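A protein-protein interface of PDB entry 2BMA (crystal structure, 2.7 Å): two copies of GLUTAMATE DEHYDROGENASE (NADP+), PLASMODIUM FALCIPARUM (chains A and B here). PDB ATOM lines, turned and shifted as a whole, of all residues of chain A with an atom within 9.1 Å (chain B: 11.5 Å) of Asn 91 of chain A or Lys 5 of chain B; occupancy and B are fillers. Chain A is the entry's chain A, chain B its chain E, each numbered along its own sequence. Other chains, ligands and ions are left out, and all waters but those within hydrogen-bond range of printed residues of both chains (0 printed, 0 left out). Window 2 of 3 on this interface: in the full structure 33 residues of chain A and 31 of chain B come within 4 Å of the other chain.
The side-chain amide oxygen of Gln 94 of chain A sits at hydrogen-bond distance from the guanidinium group of Arg 10 of chain B (2.6 Å). The side-chain amino group of Lys 5 of chain B sits at hydrogen-bond distance from the backbone carbonyl oxygen of Asn 91 of chain A (3.5 Å).
OD2 of Asp 6 of chain B lies within hydrogen-bond range of N of Gly 9 of chain B, 3.2 Å away. The side-chain carboxylate of Asp 89 of chain A sits at hydrogen-bond distance from the backbone NH of Asn 91 of chain A (2.7 Å). The guanidinium group (NE) of Arg 10 of chain B lies within hydrogen-bond range of the side-chain hydroxyl (OG1) of Thr 8 of chain B (3.1 Å). The side-chain carboxylate (OD2) of Asp 89 of chain A is in hydrogen-bond range of the backbone NH (N) of Val 93 of chain A, at 2.9 Å. The side-chain carboxylate (OD2) of Asp 89 of chain A lies within hydrogen-bond range of the backbone NH (N) of Gly 92 of chain A, at 2.8 Å. The guanidinium group of Arg 10 of chain B lies within hydrogen-bond range of the backbone carbonyl oxygen of Ile 465 of chain B, 2.9 Å away.
Arg 10 of chain B touches Leu 88 of chain A (CG to CD2, 3.4 Å). Gly 92 of chain A touches Gly 9 of chain B (O to O, 3.5 Å). Gly 92 of chain A touches Arg 10 of chain B (O to CA, 3.6 Å). O of Arg 10 of chain B touches CG1 of Val 93 of chain A, 3.9 Å away. Phe 11 of chain B touches Gln 94 of chain A.
Of chain B, only Lys 5 comes within 4 Å of Asn 91 of chain A. Lys 5 of chain B touches just one residue of chain A: Asn 91 (3.5 Å). Asp 89 of chain A touches none of the printed residues of chain B. Of chain B, only Gly 9 (3.5 Å) and Arg 10 (3.6 Å) come within 4 Å of Gly 92 of chain A. No residue of chain A comes within 4 Å of Leu 4 of chain B. Of the printed residues of chain A, Gly 9 of chain B touches Gly 92. Of the printed residues of chain A, Arg 10 of chain B touches Leu 88 (3.4 Å), Gly 92 (3.6 Å), Val 93 (3.9 Å) and Gln 94 (2.6 Å). Of the printed residues of chain B, Leu 88 of chain A touches Arg 10. Glu 162 of chain A touches none of the printed residues of chain B.
Printed residues of chain A that touch a printed residue of chain B: Leu 88, Asn 91, Gly 92, Val 93 and Gln 94. Hydrophobic or aromatic side chains of chain A within 4 Å of the printed part of chain B: Leu 88 and Val 93. Of the 22 printed residues of chain B, 4 touch a printed residue of chain A. Printed residues of chain B that touch a printed residue of chain A: Lys 5, Gly 9, Arg 10 and Phe 11. Hydrophobic or aromatic side chains of chain B within 4 Å of the printed part of chain A: Phe 11.
No position is printed for both chains.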
ATOM      1  N   TRP A  87      -4.417  10.864 -30.325  1.00  0.00           N
ATOM      2  CA  TRP A  87      -4.404  12.316 -30.306  1.00  0.00           C
ATOM      3  C   TRP A  87      -5.794  12.872 -30.594  1.00  0.00           C
ATOM      4  O   TRP A  87      -6.585  12.257 -31.302  1.00  0.00           O
ATOM      5  CB  TRP A  87      -3.427  12.829 -31.366  1.00  0.00           C
ATOM      6  CG  TRP A  87      -3.632  12.206 -32.734  1.00  0.00           C
ATOM      7  CD1 TRP A  87      -3.344  10.920 -33.103  1.00  0.00           C
ATOM      8  CD2 TRP A  87      -4.192  12.839 -33.894  1.00  0.00           C
ATOM      9  NE1 TRP A  87      -3.694  10.713 -34.420  1.00  0.00           N
ATOM     10  CE2 TRP A  87      -4.217  11.871 -34.929  1.00  0.00           C
ATOM     11  CE3 TRP A  87      -4.676  14.129 -34.160  1.00  0.00           C
ATOM     12  CZ2 TRP A  87      -4.710  12.149 -36.210  1.00  0.00           C
ATOM     13  CZ3 TRP A  87      -5.163  14.411 -35.434  1.00  0.00           C
ATOM     14  CH2 TRP A  87      -5.178  13.421 -36.444  1.00  0.00           C
ATOM     15  N   LEU A  88      -6.088  14.041 -30.038  1.00  0.00           N
ATOM     16  CA  LEU A  88      -7.368  14.684 -30.276  1.00  0.00           C
ATOM     17  C   LEU A  88      -7.261  15.406 -31.622  1.00  0.00           C
ATOM     18  O   LEU A  88      -6.235  16.027 -31.907  1.00  0.00           O
ATOM     19  CB  LEU A  88      -7.668  15.709 -29.176  1.00  0.00           C
ATOM     20  CG  LEU A  88      -7.929  15.241 -27.741  1.00  0.00           C
ATOM     21  CD1 LEU A  88      -8.135  16.432 -26.857  1.00  0.00           C
ATOM     22  CD2 LEU A  88      -9.147  14.348 -27.701  1.00  0.00           C
ATOM     23  N   ASP A  89      -8.293  15.305 -32.462  1.00  0.00           N
ATOM     24  CA  ASP A  89      -8.262  16.011 -33.738  1.00  0.00           C
ATOM     25  C   ASP A  89      -8.847  17.389 -33.472  1.00  0.00           C
ATOM     26  O   ASP A  89      -9.116  17.735 -32.317  1.00  0.00           O
ATOM     27  CB  ASP A  89      -9.038  15.259 -34.839  1.00  0.00           C
ATOM     28  CG  ASP A  89     -10.551  15.277 -34.654  1.00  0.00           C
ATOM     29  OD1 ASP A  89     -11.226  14.540 -35.414  1.00  0.00           O
ATOM     30  OD2 ASP A  89     -11.069  16.009 -33.786  1.00  0.00           O
ATOM     31  N   ASP A  90      -9.031  18.189 -34.512  1.00  0.00           N
ATOM     32  CA  ASP A  90      -9.555  19.527 -34.289  1.00  0.00           C
ATOM     33  C   ASP A  90     -11.006  19.550 -33.840  1.00  0.00           C
ATOM     34  O   ASP A  90     -11.426  20.461 -33.147  1.00  0.00           O
ATOM     35  CB  ASP A  90      -9.372  20.378 -35.544  1.00  0.00           C
ATOM     36  CG  ASP A  90      -7.950  20.864 -35.702  1.00  0.00           C
ATOM     37  OD1 ASP A  90      -7.568  21.206 -36.845  1.00  0.00           O
ATOM     38  OD2 ASP A  90      -7.221  20.915 -34.682  1.00  0.00           O
ATOM     39  N   ASN A  91     -11.775  18.544 -34.224  1.00  0.00           N
ATOM     40  CA  ASN A  91     -13.169  18.513 -33.830  1.00  0.00           C
ATOM     41  C   ASN A  91     -13.295  18.028 -32.405  1.00  0.00           C
ATOM     42  O   ASN A  91     -14.400  17.950 -31.872  1.00  0.00           O
ATOM     43  CB  ASN A  91     -13.956  17.598 -34.758  1.00  0.00           C
ATOM     44  CG  ASN A  91     -14.026  18.129 -36.177  1.00  0.00           C
ATOM     45  OD1 ASN A  91     -14.196  17.370 -37.119  1.00  0.00           O
ATOM     46  ND2 ASN A  91     -13.907  19.441 -36.332  1.00  0.00           N
ATOM     47  N   GLY A  92     -12.161  17.705 -31.789  1.00  0.00           N
ATOM     48  CA  GLY A  92     -12.173  17.216 -30.426  1.00  0.00           C
ATOM     49  C   GLY A  92     -12.269  15.700 -30.335  1.00  0.00           C
ATOM     50  O   GLY A  92     -12.192  15.134 -29.240  1.00  0.00           O
ATOM     51  N   VAL A  93     -12.437  15.032 -31.475  1.00  0.00           N
ATOM     52  CA  VAL A  93     -12.535  13.577 -31.484  1.00  0.00           C
ATOM     53  C   VAL A  93     -11.179  12.910 -31.251  1.00  0.00           C
ATOM     54  O   VAL A  93     -10.169  13.325 -31.819  1.00  0.00           O
ATOM     55  CB  VAL A  93     -13.110  13.070 -32.820  1.00  0.00           C
ATOM     56  CG1 VAL A  93     -13.195  11.544 -32.805  1.00  0.00           C
ATOM     57  CG2 VAL A  93     -14.507  13.678 -33.052  1.00  0.00           C
ATOM     58  N   GLN A  94     -11.161  11.872 -30.416  1.00  0.00           N
ATOM     59  CA  GLN A  94      -9.922  11.157 -30.130  1.00  0.00           C
ATOM     60  C   GLN A  94      -9.592  10.221 -31.277  1.00  0.00           C
ATOM     61  O   GLN A  94     -10.411   9.399 -31.657  1.00  0.00           O
ATOM     62  CB  GLN A  94     -10.045  10.357 -28.840  1.00  0.00           C
ATOM     63  CG  GLN A  94      -8.780   9.610 -28.498  1.00  0.00           C
ATOM     64  CD  GLN A  94      -8.896   8.866 -27.201  1.00  0.00           C
ATOM     65  OE1 GLN A  94      -9.113   9.469 -26.151  1.00  0.00           O
ATOM     66  NE2 GLN A  94      -8.755   7.547 -27.259  1.00  0.00           N
ATOM     67  N   ARG A  95      -8.384  10.351 -31.814  1.00  0.00           N
ATOM     68  CA  ARG A  95      -7.921   9.550 -32.947  1.00  0.00           C
ATOM     69  C   ARG A  95      -6.818   8.565 -32.580  1.00  0.00           C
ATOM     70  O   ARG A  95      -6.186   8.704 -31.544  1.00  0.00           O
ATOM     71  CB  ARG A  95      -7.404  10.477 -34.042  1.00  0.00           C
ATOM     72  CG  ARG A  95      -8.388  11.542 -34.460  1.00  0.00           C
ATOM     73  CD  ARG A  95      -9.582  10.967 -35.217  1.00  0.00           C
ATOM     74  NE  ARG A  95      -9.852  11.742 -36.429  1.00  0.00           N
ATOM     75  CZ  ARG A  95      -9.093  11.713 -37.527  1.00  0.00           C
ATOM     76  NH1 ARG A  95      -8.016  10.936 -37.576  1.00  0.00           N
ATOM     77  NH2 ARG A  95      -9.403  12.470 -38.579  1.00  0.00           N
ATOM     78  N   SER A 159      -4.617  20.043 -39.828  1.00  0.00           N
ATOM     79  CA  SER A 159      -4.277  21.436 -39.557  1.00  0.00           C
ATOM     80  C   SER A 159      -2.871  21.435 -38.997  1.00  0.00           C
ATOM     81  O   SER A 159      -2.318  20.377 -38.685  1.00  0.00           O
ATOM     82  CB  SER A 159      -5.227  22.043 -38.520  1.00  0.00           C
ATOM     83  OG  SER A 159      -5.104  21.405 -37.266  1.00  0.00           O
ATOM     84  N   GLU A 162      -3.096  19.996 -35.615  1.00  0.00           N
ATOM     85  CA  GLU A 162      -3.234  18.558 -35.559  1.00  0.00           C
ATOM     86  C   GLU A 162      -1.883  17.865 -35.709  1.00  0.00           C
ATOM     87  O   GLU A 162      -1.612  16.871 -35.028  1.00  0.00           O
ATOM     88  CB  GLU A 162      -4.205  18.102 -36.639  1.00  0.00           C
ATOM     89  CG  GLU A 162      -5.643  18.251 -36.201  1.00  0.00           C
ATOM     90  CD  GLU A 162      -6.628  18.040 -37.326  1.00  0.00           C
ATOM     91  OE1 GLU A 162      -7.790  17.687 -37.024  1.00  0.00           O
ATOM     92  OE2 GLU A 162      -6.246  18.234 -38.502  1.00  0.00           O
ATOM     93  N   LYS A 165      -0.206  18.151 -32.267  1.00  0.00           N
ATOM     94  CA  LYS A 165      -0.804  17.219 -31.314  1.00  0.00           C
ATOM     95  C   LYS A 165      -0.332  15.806 -31.607  1.00  0.00           C
ATOM     96  O   LYS A 165      -0.061  15.036 -30.681  1.00  0.00           O
ATOM     97  CB  LYS A 165      -2.330  17.224 -31.406  1.00  0.00           C
ATOM     98  CG  LYS A 165      -3.031  18.518 -31.075  1.00  0.00           C
ATOM     99  CD  LYS A 165      -4.526  18.319 -31.316  1.00  0.00           C
ATOM    100  CE  LYS A 165      -5.328  19.603 -31.196  1.00  0.00           C
ATOM    101  NZ  LYS A 165      -6.367  19.654 -32.260  1.00  0.00           N
ATOM    102  N   LEU B   4     -24.284  12.334 -30.479  1.00  0.00           N
ATOM    103  CA  LEU B   4     -23.093  12.301 -31.379  1.00  0.00           C
ATOM    104  C   LEU B   4     -21.804  11.998 -30.611  1.00  0.00           C
ATOM    105  O   LEU B   4     -20.904  11.340 -31.134  1.00  0.00           O
ATOM    106  CB  LEU B   4     -22.952  13.644 -32.119  1.00  0.00           C
ATOM    107  CG  LEU B   4     -22.665  13.620 -33.633  1.00  0.00           C
ATOM    108  CD1 LEU B   4     -22.644  15.046 -34.186  1.00  0.00           C
ATOM    109  CD2 LEU B   4     -21.342  12.920 -33.903  1.00  0.00           C
ATOM    110  N   LYS B   5     -21.712  12.466 -29.368  1.00  0.00           N
ATOM    111  CA  LYS B   5     -20.508  12.243 -28.559  1.00  0.00           C
ATOM    112  C   LYS B   5     -20.768  11.988 -27.064  1.00  0.00           C
ATOM    113  O   LYS B   5     -21.732  12.509 -26.488  1.00  0.00           O
ATOM    114  CB  LYS B   5     -19.567  13.443 -28.719  1.00  0.00           C
ATOM    115  CG  LYS B   5     -19.167  13.674 -30.165  1.00  0.00           C
ATOM    116  CD  LYS B   5     -18.405  14.976 -30.372  1.00  0.00           C
ATOM    117  CE  LYS B   5     -18.233  15.253 -31.862  1.00  0.00           C
ATOM    118  NZ  LYS B   5     -17.569  16.558 -32.116  1.00  0.00           N
ATOM    119  N   ASP B   6     -19.903  11.181 -26.441  1.00  0.00           N
ATOM    120  CA  ASP B   6     -20.025  10.873 -25.013  1.00  0.00           C
ATOM    121  C   ASP B   6     -19.771  12.135 -24.194  1.00  0.00           C
ATOM    122  O   ASP B   6     -19.662  13.233 -24.748  1.00  0.00           O
ATOM    123  CB  ASP B   6     -19.021   9.791 -24.595  1.00  0.00           C
ATOM    124  CG  ASP B   6     -17.584  10.286 -24.610  1.00  0.00           C
ATOM    125  OD1 ASP B   6     -16.916  10.174 -23.557  1.00  0.00           O
ATOM    126  OD2 ASP B   6     -17.129  10.778 -25.675  1.00  0.00           O
ATOM    127  N   LYS B   7     -19.664  11.970 -22.878  1.00  0.00           N
ATOM    128  CA  LYS B   7     -19.430  13.100 -21.982  1.00  0.00           C
ATOM    129  C   LYS B   7     -18.068  13.742 -22.212  1.00  0.00           C
ATOM    130  O   LYS B   7     -17.912  14.946 -22.046  1.00  0.00           O
ATOM    131  CB  LYS B   7     -19.530  12.644 -20.524  1.00  0.00           C
ATOM    132  CG  LYS B   7     -20.829  11.919 -20.202  1.00  0.00           C
ATOM    133  CD  LYS B   7     -20.771  11.194 -18.857  1.00  0.00           C
ATOM    134  CE  LYS B   7     -21.837  10.085 -18.772  1.00  0.00           C
ATOM    135  NZ  LYS B   7     -21.785   9.342 -17.467  1.00  0.00           N
ATOM    136  N   THR B   8     -17.085  12.938 -22.604  1.00  0.00           N
ATOM    137  CA  THR B   8     -15.736  13.443 -22.817  1.00  0.00           C
ATOM    138  C   THR B   8     -15.586  14.163 -24.160  1.00  0.00           C
ATOM    139  O   THR B   8     -14.659  14.944 -24.362  1.00  0.00           O
ATOM    140  CB  THR B   8     -14.704  12.285 -22.730  1.00  0.00           C
ATOM    141  OG1 THR B   8     -13.457  12.777 -22.203  1.00  0.00           O
ATOM    142  CG2 THR B   8     -14.463  11.679 -24.106  1.00  0.00           C
ATOM    143  N   GLY B   9     -16.503  13.902 -25.080  1.00  0.00           N
ATOM    144  CA  GLY B   9     -16.414  14.536 -26.380  1.00  0.00           C
ATOM    145  C   GLY B   9     -15.416  13.849 -27.291  1.00  0.00           C
ATOM    146  O   GLY B   9     -15.459  14.034 -28.502  1.00  0.00           O
ATOM    147  N   ARG B  10     -14.523  13.053 -26.710  1.00  0.00           N
ATOM    148  CA  ARG B  10     -13.503  12.325 -27.467  1.00  0.00           C
ATOM    149  C   ARG B  10     -14.083  11.109 -28.194  1.00  0.00           C
ATOM    150  O   ARG B  10     -13.412  10.509 -29.036  1.00  0.00           O
ATOM    151  CB  ARG B  10     -12.365  11.861 -26.529  1.00  0.00           C
ATOM    152  CG  ARG B  10     -11.647  12.997 -25.796  1.00  0.00           C
ATOM    153  CD  ARG B  10     -10.457  12.548 -24.941  1.00  0.00           C
ATOM    154  NE  ARG B  10     -10.819  12.112 -23.589  1.00  0.00           N
ATOM    155  CZ  ARG B  10     -10.903  10.839 -23.222  1.00  0.00           C
ATOM    156  NH1 ARG B  10     -10.655   9.894 -24.113  1.00  0.00           N
ATOM    157  NH2 ARG B  10     -11.205  10.505 -21.973  1.00  0.00           N
ATOM    158  N   PHE B  11     -15.327  10.751 -27.887  1.00  0.00           N
ATOM    159  CA  PHE B  11     -15.930   9.579 -28.515  1.00  0.00           C
ATOM    160  C   PHE B  11     -17.315   9.756 -29.126  1.00  0.00           C
ATOM    161  O   PHE B  11     -18.230  10.284 -28.494  1.00  0.00           O
ATOM    162  CB  PHE B  11     -15.960   8.416 -27.514  1.00  0.00           C
ATOM    163  CG  PHE B  11     -14.605   8.022 -27.022  1.00  0.00           C
ATOM    164  CD1 PHE B  11     -14.156   8.432 -25.775  1.00  0.00           C
ATOM    165  CD2 PHE B  11     -13.746   7.298 -27.840  1.00  0.00           C
ATOM    166  CE1 PHE B  11     -12.862   8.126 -25.358  1.00  0.00           C
ATOM    167  CE2 PHE B  11     -12.461   6.992 -27.432  1.00  0.00           C
ATOM    168  CZ  PHE B  11     -12.016   7.405 -26.194  1.00  0.00           C
ATOM    169  N   VAL B  12     -17.459   9.279 -30.358  1.00  0.00           N
ATOM    170  CA  VAL B  12     -18.721   9.351 -31.090  1.00  0.00           C
ATOM    171  C   VAL B  12     -19.771   8.284 -30.715  1.00  0.00           C
ATOM    172  O   VAL B  12     -19.509   7.078 -30.789  1.00  0.00           O
ATOM    173  CB  VAL B  12     -18.455   9.282 -32.598  1.00  0.00           C
ATOM    174  CG1 VAL B  12     -19.700   8.795 -33.322  1.00  0.00           C
ATOM    175  CG2 VAL B  12     -18.033  10.663 -33.105  1.00  0.00           C
ATOM    176  N   VAL B  13     -20.958   8.751 -30.320  1.00  0.00           N
ATOM    177  CA  VAL B  13     -22.076   7.877 -29.932  1.00  0.00           C
ATOM    178  C   VAL B  13     -22.716   7.329 -31.201  1.00  0.00           C
ATOM    179  O   VAL B  13     -22.449   7.822 -32.287  1.00  0.00           O
ATOM    180  CB  VAL B  13     -23.182   8.652 -29.153  1.00  0.00           C
ATOM    181  CG1 VAL B  13     -24.226   7.683 -28.603  1.00  0.00           C
ATOM    182  CG2 VAL B  13     -22.566   9.447 -28.021  1.00  0.00           C
ATOM    183  N   LEU B  14     -23.565   6.318 -31.073  1.00  0.00           N
ATOM    184  CA  LEU B  14     -24.217   5.752 -32.250  1.00  0.00           C
ATOM    185  C   LEU B  14     -25.726   5.851 -32.022  1.00  0.00           C
ATOM    186  O   LEU B  14     -26.434   4.847 -32.099  1.00  0.00           O
ATOM    187  CB  LEU B  14     -23.789   4.285 -32.426  1.00  0.00           C
ATOM    188  CG  LEU B  14     -23.647   3.701 -33.832  1.00  0.00           C
ATOM    189  CD1 LEU B  14     -22.661   4.522 -34.636  1.00  0.00           C
ATOM    190  CD2 LEU B  14     -23.195   2.250 -33.734  1.00  0.00           C
ATOM    191  N   ASP B  15     -26.199   7.069 -31.755  1.00  0.00           N
ATOM    192  CA  ASP B  15     -27.606   7.353 -31.460  1.00  0.00           C
ATOM    193  C   ASP B  15     -28.510   6.143 -31.293  1.00  0.00           C
ATOM    194  O   ASP B  15     -29.021   5.590 -32.265  1.00  0.00           O
ATOM    195  CB  ASP B  15     -28.234   8.287 -32.494  1.00  0.00           C
ATOM    196  CG  ASP B  15     -29.512   8.927 -31.969  1.00  0.00           C
ATOM    197  OD1 ASP B  15     -30.426   8.169 -31.581  1.00  0.00           O
ATOM    198  OD2 ASP B  15     -29.605  10.176 -31.925  1.00  0.00           O
ATOM    199  N   LYS B  16     -28.722   5.771 -30.034  1.00  0.00           N
ATOM    200  CA  LYS B  16     -29.536   4.615 -29.674  1.00  0.00           C
ATOM    201  C   LYS B  16     -31.041   4.844 -29.877  1.00  0.00           C
ATOM    202  O   LYS B  16     -31.834   3.902 -29.764  1.00  0.00           O
ATOM    203  CB  LYS B  16     -29.233   4.201 -28.219  1.00  0.00           C
ATOM    204  CG  LYS B  16     -29.942   2.939 -27.727  1.00  0.00           C
ATOM    205  CD  LYS B  16     -29.522   2.620 -26.287  1.00  0.00           C
ATOM    206  CE  LYS B  16     -30.344   1.486 -25.663  1.00  0.00           C
ATOM    207  NZ  LYS B  16     -30.102   1.359 -24.172  1.00  0.00           N
ATOM    208  N   ASN B  17     -31.441   6.080 -30.171  1.00  0.00           N
ATOM    209  CA  ASN B  17     -32.857   6.336 -30.396  1.00  0.00           C
ATOM    210  C   ASN B  17     -33.147   6.550 -31.885  1.00  0.00           C
ATOM    211  O   ASN B  17     -34.222   7.021 -32.269  1.00  0.00           O
ATOM    212  CB  ASN B  17     -33.364   7.520 -29.545  1.00  0.00           C
ATOM    213  CG  ASN B  17     -32.567   8.792 -29.760  1.00  0.00           C
ATOM    214  OD1 ASN B  17     -31.460   8.948 -29.227  1.00  0.00           O
ATOM    215  ND2 ASN B  17     -33.120   9.709 -30.551  1.00  0.00           N
ATOM    216  N   GLU B  64     -23.951   0.579 -24.585  1.00  0.00           N
ATOM    217  CA  GLU B  64     -23.024   1.700 -24.551  1.00  0.00           C
ATOM    218  C   GLU B  64     -22.211   1.738 -25.841  1.00  0.00           C
ATOM    219  O   GLU B  64     -21.070   1.278 -25.882  1.00  0.00           O
ATOM    220  CB  GLU B  64     -22.080   1.569 -23.354  1.00  0.00           C
ATOM    221  CG  GLU B  64     -22.714   1.856 -22.004  1.00  0.00           C
ATOM    222  CD  GLU B  64     -23.396   3.223 -21.957  1.00  0.00           C
ATOM    223  OE1 GLU B  64     -24.641   3.239 -22.013  1.00  0.00           O
ATOM    224  OE2 GLU B  64     -22.703   4.275 -21.880  1.00  0.00           O
ATOM    225  N   PRO B  65     -22.792   2.295 -26.916  1.00  0.00           N
ATOM    226  CA  PRO B  65     -22.121   2.395 -28.217  1.00  0.00           C
ATOM    227  C   PRO B  65     -20.779   3.115 -28.120  1.00  0.00           C
ATOM    228  O   PRO B  65     -19.930   2.995 -29.011  1.00  0.00           O
ATOM    229  CB  PRO B  65     -23.120   3.176 -29.068  1.00  0.00           C
ATOM    230  CG  PRO B  65     -24.413   2.806 -28.489  1.00  0.00           C
ATOM    231  CD  PRO B  65     -24.159   2.832 -26.998  1.00  0.00           C
ATOM    232  N   LYS B  66     -20.598   3.872 -27.043  1.00  0.00           N
ATOM    233  CA  LYS B  66     -19.353   4.586 -26.864  1.00  0.00           C
ATOM    234  C   LYS B  66     -18.192   3.600 -26.784  1.00  0.00           C
ATOM    235  O   LYS B  66     -17.046   3.961 -27.082  1.00  0.00           O
ATOM    236  CB  LYS B  66     -19.400   5.445 -25.603  1.00  0.00           C
ATOM    237  CG  LYS B  66     -19.378   4.673 -24.289  1.00  0.00           C
ATOM    238  CD  LYS B  66     -19.212   5.643 -23.121  1.00  0.00           C
ATOM    239  CE  LYS B  66     -18.987   4.937 -21.800  1.00  0.00           C
ATOM    240  NZ  LYS B  66     -18.750   5.899 -20.693  1.00  0.00           N
ATOM    241  N   TYR B  67     -18.484   2.355 -26.395  1.00  0.00           N
ATOM    242  CA  TYR B  67     -17.438   1.332 -26.287  1.00  0.00           C
ATOM    243  C   TYR B  67     -17.004   0.747 -27.636  1.00  0.00           C
ATOM    244  O   TYR B  67     -16.153  -0.141 -27.685  1.00  0.00           O
ATOM    245  CB  TYR B  67     -17.877   0.213 -25.324  1.00  0.00           C
ATOM    246  CG  TYR B  67     -17.906   0.654 -23.867  1.00  0.00           C
ATOM    247  CD1 TYR B  67     -19.049   0.473 -23.075  1.00  0.00           C
ATOM    248  CD2 TYR B  67     -16.804   1.307 -23.296  1.00  0.00           C
ATOM    249  CE1 TYR B  67     -19.097   0.943 -21.757  1.00  0.00           C
ATOM    250  CE2 TYR B  67     -16.839   1.774 -21.985  1.00  0.00           C
ATOM    251  CZ  TYR B  67     -17.988   1.597 -21.220  1.00  0.00           C
ATOM    252  OH  TYR B  67     -18.027   2.118 -19.942  1.00  0.00           O
ATOM    253  N   LEU B  68     -17.579   1.254 -28.728  1.00  0.00           N
ATOM    254  CA  LEU B  68     -17.220   0.779 -30.060  1.00  0.00           C
ATOM    255  C   LEU B  68     -15.852   1.298 -30.496  1.00  0.00           C
ATOM    256  O   LEU B  68     -15.007   0.520 -30.931  1.00  0.00           O
ATOM    257  CB  LEU B  68     -18.279   1.185 -31.082  1.00  0.00           C
ATOM    258  CG  LEU B  68     -19.329   0.104 -31.316  1.00  0.00           C
ATOM    259  CD1 LEU B  68     -20.427   0.610 -32.223  1.00  0.00           C
ATOM    260  CD2 LEU B  68     -18.641  -1.109 -31.918  1.00  0.00           C
ATOM    261  N   PRO B  69     -15.615   2.624 -30.396  1.00  0.00           N
ATOM    262  CA  PRO B  69     -14.318   3.180 -30.798  1.00  0.00           C
ATOM    263  C   PRO B  69     -13.225   2.664 -29.858  1.00  0.00           C
ATOM    264  O   PRO B  69     -12.076   2.415 -30.271  1.00  0.00           O
ATOM    265  CB  PRO B  69     -14.522   4.683 -30.648  1.00  0.00           C
ATOM    266  CG  PRO B  69     -15.978   4.849 -30.823  1.00  0.00           C
ATOM    267  CD  PRO B  69     -16.546   3.705 -30.043  1.00  0.00           C
ATOM    268  N   ILE B  70     -13.602   2.487 -28.592  1.00  0.00           N
ATOM    269  CA  ILE B  70     -12.687   2.016 -27.572  1.00  0.00           C
ATOM    270  C   ILE B  70     -12.115   0.606 -27.834  1.00  0.00           C
ATOM    271  O   ILE B  70     -10.904   0.445 -27.901  1.00  0.00           O
ATOM    272  CB  ILE B  70     -13.375   2.110 -26.171  1.00  0.00           C
ATOM    273  CG1 ILE B  70     -13.675   3.581 -25.861  1.00  0.00           C
ATOM    274  CG2 ILE B  70     -12.478   1.543 -25.084  1.00  0.00           C
ATOM    275  CD1 ILE B  70     -14.593   3.806 -24.702  1.00  0.00           C
ATOM    276  N   ILE B 465     -10.972   5.446 -20.325  1.00  0.00           N
ATOM    277  CA  ILE B 465     -11.621   6.740 -20.544  1.00  0.00           C
ATOM    278  C   ILE B 465     -11.258   7.690 -19.415  1.00  0.00           C
ATOM    279  O   ILE B 465     -10.943   8.856 -19.649  1.00  0.00           O
ATOM    280  CB  ILE B 465     -13.164   6.590 -20.599  1.00  0.00           C
ATOM    281  CG1 ILE B 465     -13.589   6.039 -21.961  1.00  0.00           C
ATOM    282  CG2 ILE B 465     -13.834   7.921 -20.312  1.00  0.00           C
ATOM    283  CD1 ILE B 465     -14.982   5.475 -21.967  1.00  0.00           C
